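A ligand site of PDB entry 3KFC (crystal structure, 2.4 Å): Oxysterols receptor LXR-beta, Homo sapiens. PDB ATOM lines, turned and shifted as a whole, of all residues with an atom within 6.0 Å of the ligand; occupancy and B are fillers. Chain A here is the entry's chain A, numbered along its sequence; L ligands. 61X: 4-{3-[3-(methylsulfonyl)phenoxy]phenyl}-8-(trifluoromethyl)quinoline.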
ATOM      1  N   SER A  34      -8.742 -26.111 -15.901  1.00  0.00           N
ATOM      2  CA  SER A  34      -9.926 -25.395 -15.417  1.00  0.00           C
ATOM      3  C   SER A  34      -9.708 -23.883 -15.463  1.00  0.00           C
ATOM      4  O   SER A  34     -10.595 -23.125 -15.854  1.00  0.00           O
ATOM      5  CB  SER A  34     -10.265 -25.813 -13.980  1.00  0.00           C
ATOM      6  OG  SER A  34     -10.279 -27.222 -13.866  1.00  0.00           O
ATOM      7  N   PHE A  60     -28.256 -21.567 -17.830  1.00  0.00           N
ATOM      8  CA  PHE A  60     -28.292 -23.012 -17.898  1.00  0.00           C
ATOM      9  C   PHE A  60     -27.197 -23.553 -18.837  1.00  0.00           C
ATOM     10  O   PHE A  60     -26.620 -24.603 -18.567  1.00  0.00           O
ATOM     11  CB  PHE A  60     -29.678 -23.514 -18.312  1.00  0.00           C
ATOM     12  CG  PHE A  60     -29.776 -25.019 -18.418  1.00  0.00           C
ATOM     13  CD1 PHE A  60     -29.930 -25.800 -17.260  1.00  0.00           C
ATOM     14  CD2 PHE A  60     -29.712 -25.657 -19.647  1.00  0.00           C
ATOM     15  CE1 PHE A  60     -30.015 -27.172 -17.340  1.00  0.00           C
ATOM     16  CE2 PHE A  60     -29.793 -27.051 -19.733  1.00  0.00           C
ATOM     17  CZ  PHE A  60     -29.947 -27.809 -18.586  1.00  0.00           C
ATOM     18  N   PHE A  63     -23.775 -23.296 -16.988  1.00  0.00           N
ATOM     19  CA  PHE A  63     -23.636 -24.446 -16.097  1.00  0.00           C
ATOM     20  C   PHE A  63     -23.398 -25.747 -16.863  1.00  0.00           C
ATOM     21  O   PHE A  63     -22.560 -26.574 -16.482  1.00  0.00           O
ATOM     22  CB  PHE A  63     -24.881 -24.573 -15.216  1.00  0.00           C
ATOM     23  CG  PHE A  63     -24.626 -24.247 -13.776  1.00  0.00           C
ATOM     24  CD1 PHE A  63     -24.005 -23.056 -13.417  1.00  0.00           C
ATOM     25  CD2 PHE A  63     -25.031 -25.123 -12.777  1.00  0.00           C
ATOM     26  CE1 PHE A  63     -23.780 -22.746 -12.070  1.00  0.00           C
ATOM     27  CE2 PHE A  63     -24.806 -24.829 -11.442  1.00  0.00           C
ATOM     28  CZ  PHE A  63     -24.171 -23.641 -11.080  1.00  0.00           C
ATOM     29  N   THR A  64     -24.135 -25.916 -17.947  1.00  0.00           N
ATOM     30  CA  THR A  64     -23.934 -27.004 -18.906  1.00  0.00           C
ATOM     31  C   THR A  64     -22.495 -27.085 -19.434  1.00  0.00           C
ATOM     32  O   THR A  64     -21.927 -28.182 -19.559  1.00  0.00           O
ATOM     33  CB  THR A  64     -25.010 -26.879 -20.034  1.00  0.00           C
ATOM     34  OG1 THR A  64     -26.116 -27.741 -19.720  1.00  0.00           O
ATOM     35  CG2 THR A  64     -24.497 -27.203 -21.378  1.00  0.00           C
ATOM     36  N   GLU A  65     -21.892 -25.923 -19.689  1.00  0.00           N
ATOM     37  CA  GLU A  65     -20.500 -25.827 -20.136  1.00  0.00           C
ATOM     38  C   GLU A  65     -19.499 -26.242 -19.061  1.00  0.00           C
ATOM     39  O   GLU A  65     -18.471 -26.856 -19.372  1.00  0.00           O
ATOM     40  CB  GLU A  65     -20.187 -24.424 -20.674  1.00  0.00           C
ATOM     41  CG  GLU A  65     -20.806 -24.165 -22.045  1.00  0.00           C
ATOM     42  CD  GLU A  65     -20.772 -22.706 -22.483  1.00  0.00           C
ATOM     43  OE1 GLU A  65     -19.819 -21.958 -22.134  1.00  0.00           O
ATOM     44  OE2 GLU A  65     -21.723 -22.307 -23.195  1.00  0.00           O
ATOM     45  N   LEU A  66     -19.799 -25.913 -17.800  1.00  0.00           N
ATOM     46  CA  LEU A  66     -18.965 -26.282 -16.657  1.00  0.00           C
ATOM     47  C   LEU A  66     -18.935 -27.799 -16.485  1.00  0.00           C
ATOM     48  O   LEU A  66     -17.890 -28.374 -16.147  1.00  0.00           O
ATOM     49  CB  LEU A  66     -19.414 -25.582 -15.371  1.00  0.00           C
ATOM     50  CG  LEU A  66     -19.547 -24.048 -15.356  1.00  0.00           C
ATOM     51  CD1 LEU A  66     -20.033 -23.521 -14.011  1.00  0.00           C
ATOM     52  CD2 LEU A  66     -18.277 -23.341 -15.776  1.00  0.00           C
ATOM     53  N   ALA A  67     -20.068 -28.445 -16.758  1.00  0.00           N
ATOM     54  CA  ALA A  67     -20.185 -29.894 -16.627  1.00  0.00           C
ATOM     55  C   ALA A  67     -19.470 -30.599 -17.770  1.00  0.00           C
ATOM     56  O   ALA A  67     -18.785 -31.587 -17.546  1.00  0.00           O
ATOM     57  CB  ALA A  67     -21.654 -30.311 -16.534  1.00  0.00           C
ATOM     58  N   ILE A  69     -16.872 -29.452 -19.454  1.00  0.00           N
ATOM     59  CA  ILE A  69     -15.477 -29.327 -19.028  1.00  0.00           C
ATOM     60  C   ILE A  69     -15.104 -30.390 -18.000  1.00  0.00           C
ATOM     61  O   ILE A  69     -14.085 -31.045 -18.128  1.00  0.00           O
ATOM     62  CB  ILE A  69     -15.169 -27.892 -18.502  1.00  0.00           C
ATOM     63  CG1 ILE A  69     -15.083 -26.903 -19.669  1.00  0.00           C
ATOM     64  CG2 ILE A  69     -13.872 -27.898 -17.668  1.00  0.00           C
ATOM     65  CD1 ILE A  69     -15.255 -25.421 -19.264  1.00  0.00           C
ATOM     66  N   SER A  70     -15.945 -30.580 -16.980  1.00  0.00           N
ATOM     67  CA  SER A  70     -15.688 -31.568 -15.936  1.00  0.00           C
ATOM     68  C   SER A  70     -15.670 -33.008 -16.481  1.00  0.00           C
ATOM     69  O   SER A  70     -14.754 -33.783 -16.149  1.00  0.00           O
ATOM     70  CB  SER A  70     -16.710 -31.416 -14.822  1.00  0.00           C
ATOM     71  OG  SER A  70     -16.318 -32.142 -13.672  1.00  0.00           O
ATOM     72  N   GLU A  73     -12.315 -33.567 -18.285  1.00  0.00           N
ATOM     73  CA  GLU A  73     -11.336 -33.608 -17.202  1.00  0.00           C
ATOM     74  C   GLU A  73     -11.328 -34.948 -16.461  1.00  0.00           C
ATOM     75  O   GLU A  73     -10.257 -35.461 -16.119  1.00  0.00           O
ATOM     76  CB  GLU A  73     -11.584 -32.465 -16.201  1.00  0.00           C
ATOM     77  CG  GLU A  73     -11.168 -31.087 -16.722  1.00  0.00           C
ATOM     78  CD  GLU A  73     -11.286 -29.987 -15.678  1.00  0.00           C
ATOM     79  OE1 GLU A  73     -10.746 -28.890 -15.917  1.00  0.00           O
ATOM     80  OE2 GLU A  73     -11.926 -30.221 -14.631  1.00  0.00           O
ATOM     81  N   ILE A 101     -21.036 -38.224 -12.430  1.00  0.00           N
ATOM     82  CA  ILE A 101     -21.854 -37.428 -11.519  1.00  0.00           C
ATOM     83  C   ILE A 101     -21.213 -37.349 -10.110  1.00  0.00           C
ATOM     84  O   ILE A 101     -21.125 -36.274  -9.518  1.00  0.00           O
ATOM     85  CB  ILE A 101     -23.370 -37.881 -11.495  1.00  0.00           C
ATOM     86  CG1 ILE A 101     -24.243 -36.890 -10.721  1.00  0.00           C
ATOM     87  CG2 ILE A 101     -23.535 -39.326 -10.981  1.00  0.00           C
ATOM     88  CD1 ILE A 101     -24.062 -35.432 -11.122  1.00  0.00           C
ATOM     89  N   ILE A 103     -18.008 -37.955  -9.144  1.00  0.00           N
ATOM     90  CA  ILE A 103     -16.752 -37.236  -9.142  1.00  0.00           C
ATOM     91  C   ILE A 103     -16.972 -35.718  -9.254  1.00  0.00           C
ATOM     92  O   ILE A 103     -16.267 -34.940  -8.593  1.00  0.00           O
ATOM     93  CB  ILE A 103     -15.775 -37.782 -10.223  1.00  0.00           C
ATOM     94  CG1 ILE A 103     -15.493 -39.274  -9.947  1.00  0.00           C
ATOM     95  CG2 ILE A 103     -14.479 -36.990 -10.231  1.00  0.00           C
ATOM     96  CD1 ILE A 103     -14.637 -39.954 -10.989  1.00  0.00           C
ATOM     97  N   MET A 104     -17.948 -35.312 -10.058  1.00  0.00           N
ATOM     98  CA  MET A 104     -18.351 -33.905 -10.131  1.00  0.00           C
ATOM     99  C   MET A 104     -18.704 -33.295  -8.776  1.00  0.00           C
ATOM    100  O   MET A 104     -18.300 -32.159  -8.482  1.00  0.00           O
ATOM    101  CB  MET A 104     -19.544 -33.745 -11.063  1.00  0.00           C
ATOM    102  CG  MET A 104     -19.185 -33.786 -12.529  1.00  0.00           C
ATOM    103  SD  MET A 104     -20.703 -33.751 -13.487  1.00  0.00           S
ATOM    104  CE  MET A 104     -20.063 -33.833 -15.155  1.00  0.00           C
ATOM    105  N   LEU A 105     -19.463 -34.041  -7.967  1.00  0.00           N
ATOM    106  CA  LEU A 105     -19.943 -33.531  -6.682  1.00  0.00           C
ATOM    107  C   LEU A 105     -18.857 -33.524  -5.626  1.00  0.00           C
ATOM    108  O   LEU A 105     -18.759 -32.595  -4.830  1.00  0.00           O
ATOM    109  CB  LEU A 105     -21.173 -34.328  -6.228  1.00  0.00           C
ATOM    110  CG  LEU A 105     -22.351 -34.263  -7.200  1.00  0.00           C
ATOM    111  CD1 LEU A 105     -23.486 -35.186  -6.775  1.00  0.00           C
ATOM    112  CD2 LEU A 105     -22.827 -32.815  -7.407  1.00  0.00           C
ATOM    113  N   GLU A 107     -15.838 -33.025  -6.469  1.00  0.00           N
ATOM    114  CA  GLU A 107     -15.101 -31.838  -6.883  1.00  0.00           C
ATOM    115  C   GLU A 107     -15.770 -30.522  -6.487  1.00  0.00           C
ATOM    116  O   GLU A 107     -15.091 -29.572  -6.112  1.00  0.00           O
ATOM    117  CB  GLU A 107     -14.890 -31.857  -8.397  1.00  0.00           C
ATOM    118  CG  GLU A 107     -13.614 -32.500  -8.811  1.00  0.00           C
ATOM    119  CD  GLU A 107     -12.406 -31.658  -8.447  1.00  0.00           C
ATOM    120  OE1 GLU A 107     -12.303 -30.502  -8.949  1.00  0.00           O
ATOM    121  OE2 GLU A 107     -11.564 -32.163  -7.666  1.00  0.00           O
ATOM    122  N   THR A 108     -17.091 -30.474  -6.630  1.00  0.00           N
ATOM    123  CA  THR A 108     -17.908 -29.352  -6.168  1.00  0.00           C
ATOM    124  C   THR A 108     -17.681 -29.091  -4.676  1.00  0.00           C
ATOM    125  O   THR A 108     -17.397 -27.972  -4.267  1.00  0.00           O
ATOM    126  CB  THR A 108     -19.418 -29.624  -6.456  1.00  0.00           C
ATOM    127  OG1 THR A 108     -19.624 -29.753  -7.872  1.00  0.00           O
ATOM    128  CG2 THR A 108     -20.284 -28.517  -5.961  1.00  0.00           C
ATOM    129  N   ARG A 111     -14.483 -27.424  -3.762  1.00  0.00           N
ATOM    130  CA  ARG A 111     -14.388 -26.012  -4.105  1.00  0.00           C
ATOM    131  C   ARG A 111     -15.435 -25.186  -3.368  1.00  0.00           C
ATOM    132  O   ARG A 111     -15.627 -24.009  -3.661  1.00  0.00           O
ATOM    133  CB  ARG A 111     -14.526 -25.842  -5.626  1.00  0.00           C
ATOM    134  CG  ARG A 111     -13.563 -26.693  -6.431  1.00  0.00           C
ATOM    135  CD  ARG A 111     -14.096 -26.968  -7.831  1.00  0.00           C
ATOM    136  NE  ARG A 111     -13.346 -26.208  -8.834  1.00  0.00           N
ATOM    137  CZ  ARG A 111     -12.294 -26.689  -9.478  1.00  0.00           C
ATOM    138  NH1 ARG A 111     -11.876 -27.929  -9.229  1.00  0.00           N
ATOM    139  NH2 ARG A 111     -11.654 -25.951 -10.375  1.00  0.00           N
ATOM    140  N   THR A 120     -16.623 -22.408  -5.898  1.00  0.00           N
ATOM    141  CA  THR A 120     -15.775 -21.795  -6.906  1.00  0.00           C
ATOM    142  C   THR A 120     -15.453 -22.744  -8.056  1.00  0.00           C
ATOM    143  O   THR A 120     -14.636 -23.649  -7.917  1.00  0.00           O
ATOM    144  CB  THR A 120     -14.465 -21.223  -6.308  1.00  0.00           C
ATOM    145  OG1 THR A 120     -14.775 -20.107  -5.470  1.00  0.00           O
ATOM    146  CG2 THR A 120     -13.520 -20.736  -7.429  1.00  0.00           C
ATOM    147  N   PHE A 121     -16.113 -22.541  -9.193  1.00  0.00           N
ATOM    148  CA  PHE A 121     -15.772 -23.272 -10.410  1.00  0.00           C
ATOM    149  C   PHE A 121     -14.682 -22.564 -11.225  1.00  0.00           C
ATOM    150  O   PHE A 121     -14.494 -21.350 -11.118  1.00  0.00           O
ATOM    151  CB  PHE A 121     -17.029 -23.537 -11.238  1.00  0.00           C
ATOM    152  CG  PHE A 121     -18.022 -24.423 -10.549  1.00  0.00           C
ATOM    153  CD1 PHE A 121     -19.337 -24.005 -10.368  1.00  0.00           C
ATOM    154  CD2 PHE A 121     -17.642 -25.664 -10.040  1.00  0.00           C
ATOM    155  CE1 PHE A 121     -20.267 -24.813  -9.713  1.00  0.00           C
ATOM    156  CE2 PHE A 121     -18.576 -26.488  -9.381  1.00  0.00           C
ATOM    157  CZ  PHE A 121     -19.878 -26.066  -9.220  1.00  0.00           C
ATOM    158  N   LEU A 122     -13.939 -23.360 -12.008  1.00  0.00           N
ATOM    159  CA  LEU A 122     -12.783 -22.889 -12.779  1.00  0.00           C
ATOM    160  C   LEU A 122     -11.797 -22.119 -11.874  1.00  0.00           C
ATOM    161  O   LEU A 122     -11.385 -22.644 -10.834  1.00  0.00           O
ATOM    162  CB  LEU A 122     -13.218 -22.079 -14.006  1.00  0.00           C
ATOM    163  CG  LEU A 122     -14.266 -22.709 -14.962  1.00  0.00           C
ATOM    164  CD1 LEU A 122     -14.828 -21.691 -15.938  1.00  0.00           C
ATOM    165  CD2 LEU A 122     -13.728 -23.915 -15.712  1.00  0.00           C
ATOM    166  N   LYS A 123     -11.419 -20.893 -12.265  1.00  0.00           N
ATOM    167  CA  LYS A 123     -10.444 -20.092 -11.512  1.00  0.00           C
ATOM    168  C   LYS A 123     -11.034 -19.269 -10.353  1.00  0.00           C
ATOM    169  O   LYS A 123     -10.539 -19.350  -9.231  1.00  0.00           O
ATOM    170  CB  LYS A 123      -9.629 -19.187 -12.457  1.00  0.00           C
ATOM    171  CG  LYS A 123      -8.580 -18.307 -11.771  1.00  0.00           C
ATOM    172  CD  LYS A 123      -8.034 -17.223 -12.723  1.00  0.00           C
ATOM    173  CE  LYS A 123      -7.246 -16.158 -11.989  1.00  0.00           C
ATOM    174  NZ  LYS A 123      -6.768 -15.041 -12.888  1.00  0.00           N
ATOM    175  N   PHE A 132     -27.270 -21.536  -8.227  1.00  0.00           N
ATOM    176  CA  PHE A 132     -27.601 -22.872  -8.733  1.00  0.00           C
ATOM    177  C   PHE A 132     -29.058 -22.953  -9.200  1.00  0.00           C
ATOM    178  O   PHE A 132     -29.366 -23.594 -10.207  1.00  0.00           O
ATOM    179  CB  PHE A 132     -27.345 -23.941  -7.667  1.00  0.00           C
ATOM    180  CG  PHE A 132     -25.931 -24.468  -7.641  1.00  0.00           C
ATOM    181  CD1 PHE A 132     -24.848 -23.634  -7.319  1.00  0.00           C
ATOM    182  CD2 PHE A 132     -25.682 -25.815  -7.876  1.00  0.00           C
ATOM    183  CE1 PHE A 132     -23.560 -24.126  -7.275  1.00  0.00           C
ATOM    184  CE2 PHE A 132     -24.376 -26.324  -7.827  1.00  0.00           C
ATOM    185  CZ  PHE A 132     -23.319 -25.470  -7.530  1.00  0.00           C
ATOM    186  N   LEU A 137     -31.557 -25.339 -11.973  1.00  0.00           N
ATOM    187  CA  LEU A 137     -31.589 -26.594 -11.211  1.00  0.00           C
ATOM    188  C   LEU A 137     -32.629 -26.574 -10.076  1.00  0.00           C
ATOM    189  O   LEU A 137     -32.986 -25.506  -9.583  1.00  0.00           O
ATOM    190  CB  LEU A 137     -30.182 -26.983 -10.697  1.00  0.00           C
ATOM    191  CG  LEU A 137     -29.063 -27.267 -11.719  1.00  0.00           C
ATOM    192  CD1 LEU A 137     -27.718 -27.529 -11.028  1.00  0.00           C
ATOM    193  CD2 LEU A 137     -29.390 -28.439 -12.647  1.00  0.00           C
ATOM    194  N   PHE A 141     -32.360 -31.052  -5.651  1.00  0.00           N
ATOM    195  CA  PHE A 141     -31.014 -31.444  -6.026  1.00  0.00           C
ATOM    196  C   PHE A 141     -29.947 -30.532  -5.382  1.00  0.00           C
ATOM    197  O   PHE A 141     -28.960 -31.023  -4.860  1.00  0.00           O
ATOM    198  CB  PHE A 141     -30.904 -31.484  -7.565  1.00  0.00           C
ATOM    199  CG  PHE A 141     -29.555 -31.954  -8.086  1.00  0.00           C
ATOM    200  CD1 PHE A 141     -28.912 -33.058  -7.534  1.00  0.00           C
ATOM    201  CD2 PHE A 141     -28.965 -31.297  -9.156  1.00  0.00           C
ATOM    202  CE1 PHE A 141     -27.679 -33.483  -8.033  1.00  0.00           C
ATOM    203  CE2 PHE A 141     -27.745 -31.711  -9.653  1.00  0.00           C
ATOM    204  CZ  PHE A 141     -27.103 -32.808  -9.095  1.00  0.00           C
ATOM    205  N   HIS A 227     -29.827 -36.851  -8.807  1.00  0.00           N
ATOM    206  CA  HIS A 227     -29.486 -36.258 -10.096  1.00  0.00           C
ATOM    207  C   HIS A 227     -30.287 -36.837 -11.274  1.00  0.00           C
ATOM    208  O   HIS A 227     -30.663 -36.095 -12.184  1.00  0.00           O
ATOM    209  CB  HIS A 227     -27.982 -36.350 -10.364  1.00  0.00           C
ATOM    210  CG  HIS A 227     -27.582 -35.845 -11.716  1.00  0.00           C
ATOM    211  ND1 HIS A 227     -27.201 -36.690 -12.737  1.00  0.00           N
ATOM    212  CD2 HIS A 227     -27.506 -34.594 -12.212  1.00  0.00           C
ATOM    213  CE1 HIS A 227     -26.892 -35.979 -13.804  1.00  0.00           C
ATOM    214  NE2 HIS A 227     -27.071 -34.694 -13.519  1.00  0.00           N
ATOM    215  N   GLN A 230     -33.421 -35.023 -11.283  1.00  0.00           N
ATOM    216  CA  GLN A 230     -33.189 -33.668 -11.810  1.00  0.00           C
ATOM    217  C   GLN A 230     -33.205 -33.682 -13.336  1.00  0.00           C
ATOM    218  O   GLN A 230     -33.832 -32.840 -13.974  1.00  0.00           O
ATOM    219  CB  GLN A 230     -31.855 -33.100 -11.271  1.00  0.00           C
ATOM    220  CG  GLN A 230     -31.355 -31.793 -11.925  1.00  0.00           C
ATOM    221  CD  GLN A 230     -32.219 -30.570 -11.594  1.00  0.00           C
ATOM    222  OE1 GLN A 230     -31.923 -29.818 -10.649  1.00  0.00           O
ATOM    223  NE2 GLN A 230     -33.290 -30.371 -12.346  1.00  0.00           N
ATOM    224  N   VAL A 231     -32.506 -34.665 -13.914  1.00  0.00           N
ATOM    225  CA  VAL A 231     -32.497 -34.881 -15.359  1.00  0.00           C
ATOM    226  C   VAL A 231     -33.894 -35.266 -15.859  1.00  0.00           C
ATOM    227  O   VAL A 231     -34.301 -34.854 -16.948  1.00  0.00           O
ATOM    228  CB  VAL A 231     -31.440 -35.947 -15.756  1.00  0.00           C
ATOM    229  CG1 VAL A 231     -31.536 -36.307 -17.248  1.00  0.00           C
ATOM    230  CG2 VAL A 231     -30.030 -35.473 -15.420  1.00  0.00           C
ATOM    231  N   LEU A 234     -36.284 -32.275 -16.057  1.00  0.00           N
ATOM    232  CA  LEU A 234     -35.990 -31.504 -17.265  1.00  0.00           C
ATOM    233  C   LEU A 234     -36.620 -32.091 -18.526  1.00  0.00           C
ATOM    234  O   LEU A 234     -37.126 -31.352 -19.372  1.00  0.00           O
ATOM    235  CB  LEU A 234     -34.488 -31.360 -17.462  1.00  0.00           C
ATOM    236  CG  LEU A 234     -33.653 -30.614 -16.415  1.00  0.00           C
ATOM    237  CD1 LEU A 234     -32.223 -31.128 -16.486  1.00  0.00           C
ATOM    238  CD2 LEU A 234     -33.718 -29.110 -16.603  1.00  0.00           C
ATOM    239  N   LEU A 241     -30.443 -31.290 -22.672  1.00  0.00           N
ATOM    240  CA  LEU A 241     -29.002 -31.324 -22.464  1.00  0.00           C
ATOM    241  C   LEU A 241     -28.267 -31.319 -23.802  1.00  0.00           C
ATOM    242  O   LEU A 241     -28.777 -31.832 -24.798  1.00  0.00           O
ATOM    243  CB  LEU A 241     -28.598 -32.555 -21.642  1.00  0.00           C
ATOM    244  CG  LEU A 241     -28.983 -32.627 -20.162  1.00  0.00           C
ATOM    245  CD1 LEU A 241     -28.600 -33.973 -19.582  1.00  0.00           C
ATOM    246  CD2 LEU A 241     -28.345 -31.502 -19.361  1.00  0.00           C
ATOM    247  N   LEU A 245     -23.569 -34.491 -22.552  1.00  0.00           N
ATOM    248  CA  LEU A 245     -24.210 -34.797 -21.266  1.00  0.00           C
ATOM    249  C   LEU A 245     -25.421 -35.702 -21.453  1.00  0.00           C
ATOM    250  O   LEU A 245     -25.720 -36.537 -20.585  1.00  0.00           O
ATOM    251  CB  LEU A 245     -24.603 -33.507 -20.539  1.00  0.00           C
ATOM    252  CG  LEU A 245     -23.533 -32.455 -20.251  1.00  0.00           C
ATOM    253  CD1 LEU A 245     -24.099 -31.291 -19.432  1.00  0.00           C
ATOM    254  CD2 LEU A 245     -22.290 -33.043 -19.567  1.00  0.00           C
ATOM    255  N   TRP A 249     -26.018 -39.087 -19.455  1.00  0.00           N
ATOM    256  CA  TRP A 249     -27.056 -38.960 -18.407  1.00  0.00           C
ATOM    257  C   TRP A 249     -28.498 -39.370 -18.745  1.00  0.00           C
ATOM    258  O   TRP A 249     -29.282 -39.601 -17.818  1.00  0.00           O
ATOM    259  CB  TRP A 249     -27.050 -37.566 -17.771  1.00  0.00           C
ATOM    260  CG  TRP A 249     -25.834 -37.261 -16.930  1.00  0.00           C
ATOM    261  CD1 TRP A 249     -25.019 -38.167 -16.287  1.00  0.00           C
ATOM    262  CD2 TRP A 249     -25.306 -35.971 -16.620  1.00  0.00           C
ATOM    263  NE1 TRP A 249     -24.010 -37.512 -15.624  1.00  0.00           N
ATOM    264  CE2 TRP A 249     -24.169 -36.158 -15.801  1.00  0.00           C
ATOM    265  CE3 TRP A 249     -25.686 -34.665 -16.953  1.00  0.00           C
ATOM    266  CZ2 TRP A 249     -23.417 -35.101 -15.317  1.00  0.00           C
ATOM    267  CZ3 TRP A 249     -24.937 -33.602 -16.476  1.00  0.00           C
ATOM    268  CH2 TRP A 249     -23.810 -33.829 -15.655  1.00  0.00           C
HETATM  269  C1  61X L   1     -16.292 -25.768 -13.920  1.00  0.00           C
HETATM  270  F1  61X L   1     -28.028 -32.548 -15.738  1.00  0.00           F
HETATM  271  N1  61X L   1     -26.028 -31.895 -13.536  1.00  0.00           N
HETATM  272  O1  61X L   1     -14.536 -27.630 -14.289  1.00  0.00           O
HETATM  273  S1  61X L   1     -15.089 -26.846 -13.211  1.00  0.00           S
HETATM  274  C2  61X L   1     -16.016 -28.019 -12.250  1.00  0.00           C
HETATM  275  F2  61X L   1     -28.735 -31.582 -13.937  1.00  0.00           F
HETATM  276  O2  61X L   1     -14.223 -26.102 -12.322  1.00  0.00           O
HETATM  277  C3  61X L   1     -15.609 -28.432 -10.981  1.00  0.00           C
HETATM  278  F3  61X L   1     -29.299 -30.850 -15.846  1.00  0.00           F
HETATM  279  O3  61X L   1     -19.047 -29.962 -12.791  1.00  0.00           O
HETATM  280  C4  61X L   1     -16.383 -29.371 -10.283  1.00  0.00           C
HETATM  281  C5  61X L   1     -17.555 -29.917 -10.847  1.00  0.00           C
HETATM  282  C6  61X L   1     -17.930 -29.488 -12.137  1.00  0.00           C
HETATM  283  C7  61X L   1     -17.165 -28.551 -12.831  1.00  0.00           C
HETATM  284  C8  61X L   1     -20.229 -29.251 -12.788  1.00  0.00           C
HETATM  285  C9  61X L   1     -20.325 -27.863 -12.585  1.00  0.00           C
HETATM  286  C10 61X L   1     -21.579 -27.251 -12.587  1.00  0.00           C
HETATM  287  C11 61X L   1     -22.722 -28.015 -12.804  1.00  0.00           C
HETATM  288  C12 61X L   1     -22.626 -29.405 -13.037  1.00  0.00           C
HETATM  289  C13 61X L   1     -21.364 -30.021 -13.015  1.00  0.00           C
HETATM  290  C14 61X L   1     -23.823 -30.226 -13.266  1.00  0.00           C
HETATM  291  C15 61X L   1     -23.899 -31.432 -12.552  1.00  0.00           C
HETATM  292  C16 61X L   1     -25.012 -32.227 -12.713  1.00  0.00           C
HETATM  293  C17 61X L   1     -26.006 -30.744 -14.231  1.00  0.00           C
HETATM  294  C18 61X L   1     -24.905 -29.845 -14.137  1.00  0.00           C
HETATM  295  C19 61X L   1     -24.944 -28.652 -14.902  1.00  0.00           C
HETATM  296  C20 61X L   1     -26.017 -28.333 -15.742  1.00  0.00           C
HETATM  297  C21 61X L   1     -27.092 -29.215 -15.840  1.00  0.00           C
HETATM  298  C22 61X L   1     -27.079 -30.411 -15.089  1.00  0.00           C
HETATM  299  C23 61X L   1     -28.244 -31.345 -15.172  1.00  0.00           C
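N of Leu 122 lies within hydrogen-bond range of O2 of the ligand. NE2 of His 227 is in hydrogen-bond range of N1 of the ligand, at 3.0 Å. NH2 of Arg 111 lies within hydrogen-bond range of O2 of the ligand, at 3.2 Å.
The backbone carbonyl oxygen (O) of Leu 122 sits at hydrogen-bond distance from the guanidinium group (NH2) of Arg 111 (3.3 Å). The side-chain carboxylate (OE1) of Glu 107 lies within salt-bridge range of the guanidinium group (NH1) of Arg 111, at 2.6 Å. The backbone carbonyl oxygen (O) of Arg 111 is in hydrogen-bond range of the backbone NH (N) of Thr 120, 2.9 Å away. The backbone carbonyl oxygen (O) of Met 104 is in hydrogen-bond range of the side-chain hydroxyl (OG1) of Thr 108. O of Phe 132 is in hydrogen-bond range of N of Leu 137. OG of Ser 34 sits at hydrogen-bond distance from OE1 of Glu 73, 2.7 Å away. OG1 of Thr 64 lies close to O of Phe 60 (3.4 Å).
Phe 60 touches the ligand (CE1 to C21, 3.9 Å). Phe 63 touches the ligand. Thr 64 touches the ligand (N to C20, 3.8 Å). O of Leu 66 touches C7 of the ligand, 3.4 Å away. Ala 67 touches the ligand. CG2 of Ile 69 touches O1 of the ligand (3.5 Å). CB of Ser 70 touches O3 of the ligand (3.4 Å). Glu 73 touches the ligand (OE2 to O1, 3.7 Å). Ile 101 touches the ligand (CD1 to C16, 3.7 Å). Met 104 touches the ligand (O to C5, 3.3 Å). Glu 107 touches the ligand. Thr 108 touches the ligand. CD2 of Phe 121 touches C3 of the ligand, at 3.6 Å. Leu 137 touches the ligand. CG of Gln 230 touches F2 of the ligand, at 3.3 Å. CG2 of Val 231 touches F1 of the ligand, at 3.6 Å. CD1 of Leu 234 touches F3 of the ligand, at 3.0 Å. Leu 241 touches the ligand (CD2 to F3, 3.7 Å). CZ3 of Trp 249 touches F1 of the ligand, at 3.3 Å. Hydrophobic or aromatic side chains within 4 Å of the ligand: Phe 60, Phe 63, Leu 66, Ala 67, Ile 69, Ile 101, Met 104, Phe 121, Leu 122, Leu 137, His 227, Val 231, Leu 234, Leu 241 and Trp 249. The nearest printed residue that does not touch the ligand is Phe 141 (4.1 Å).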
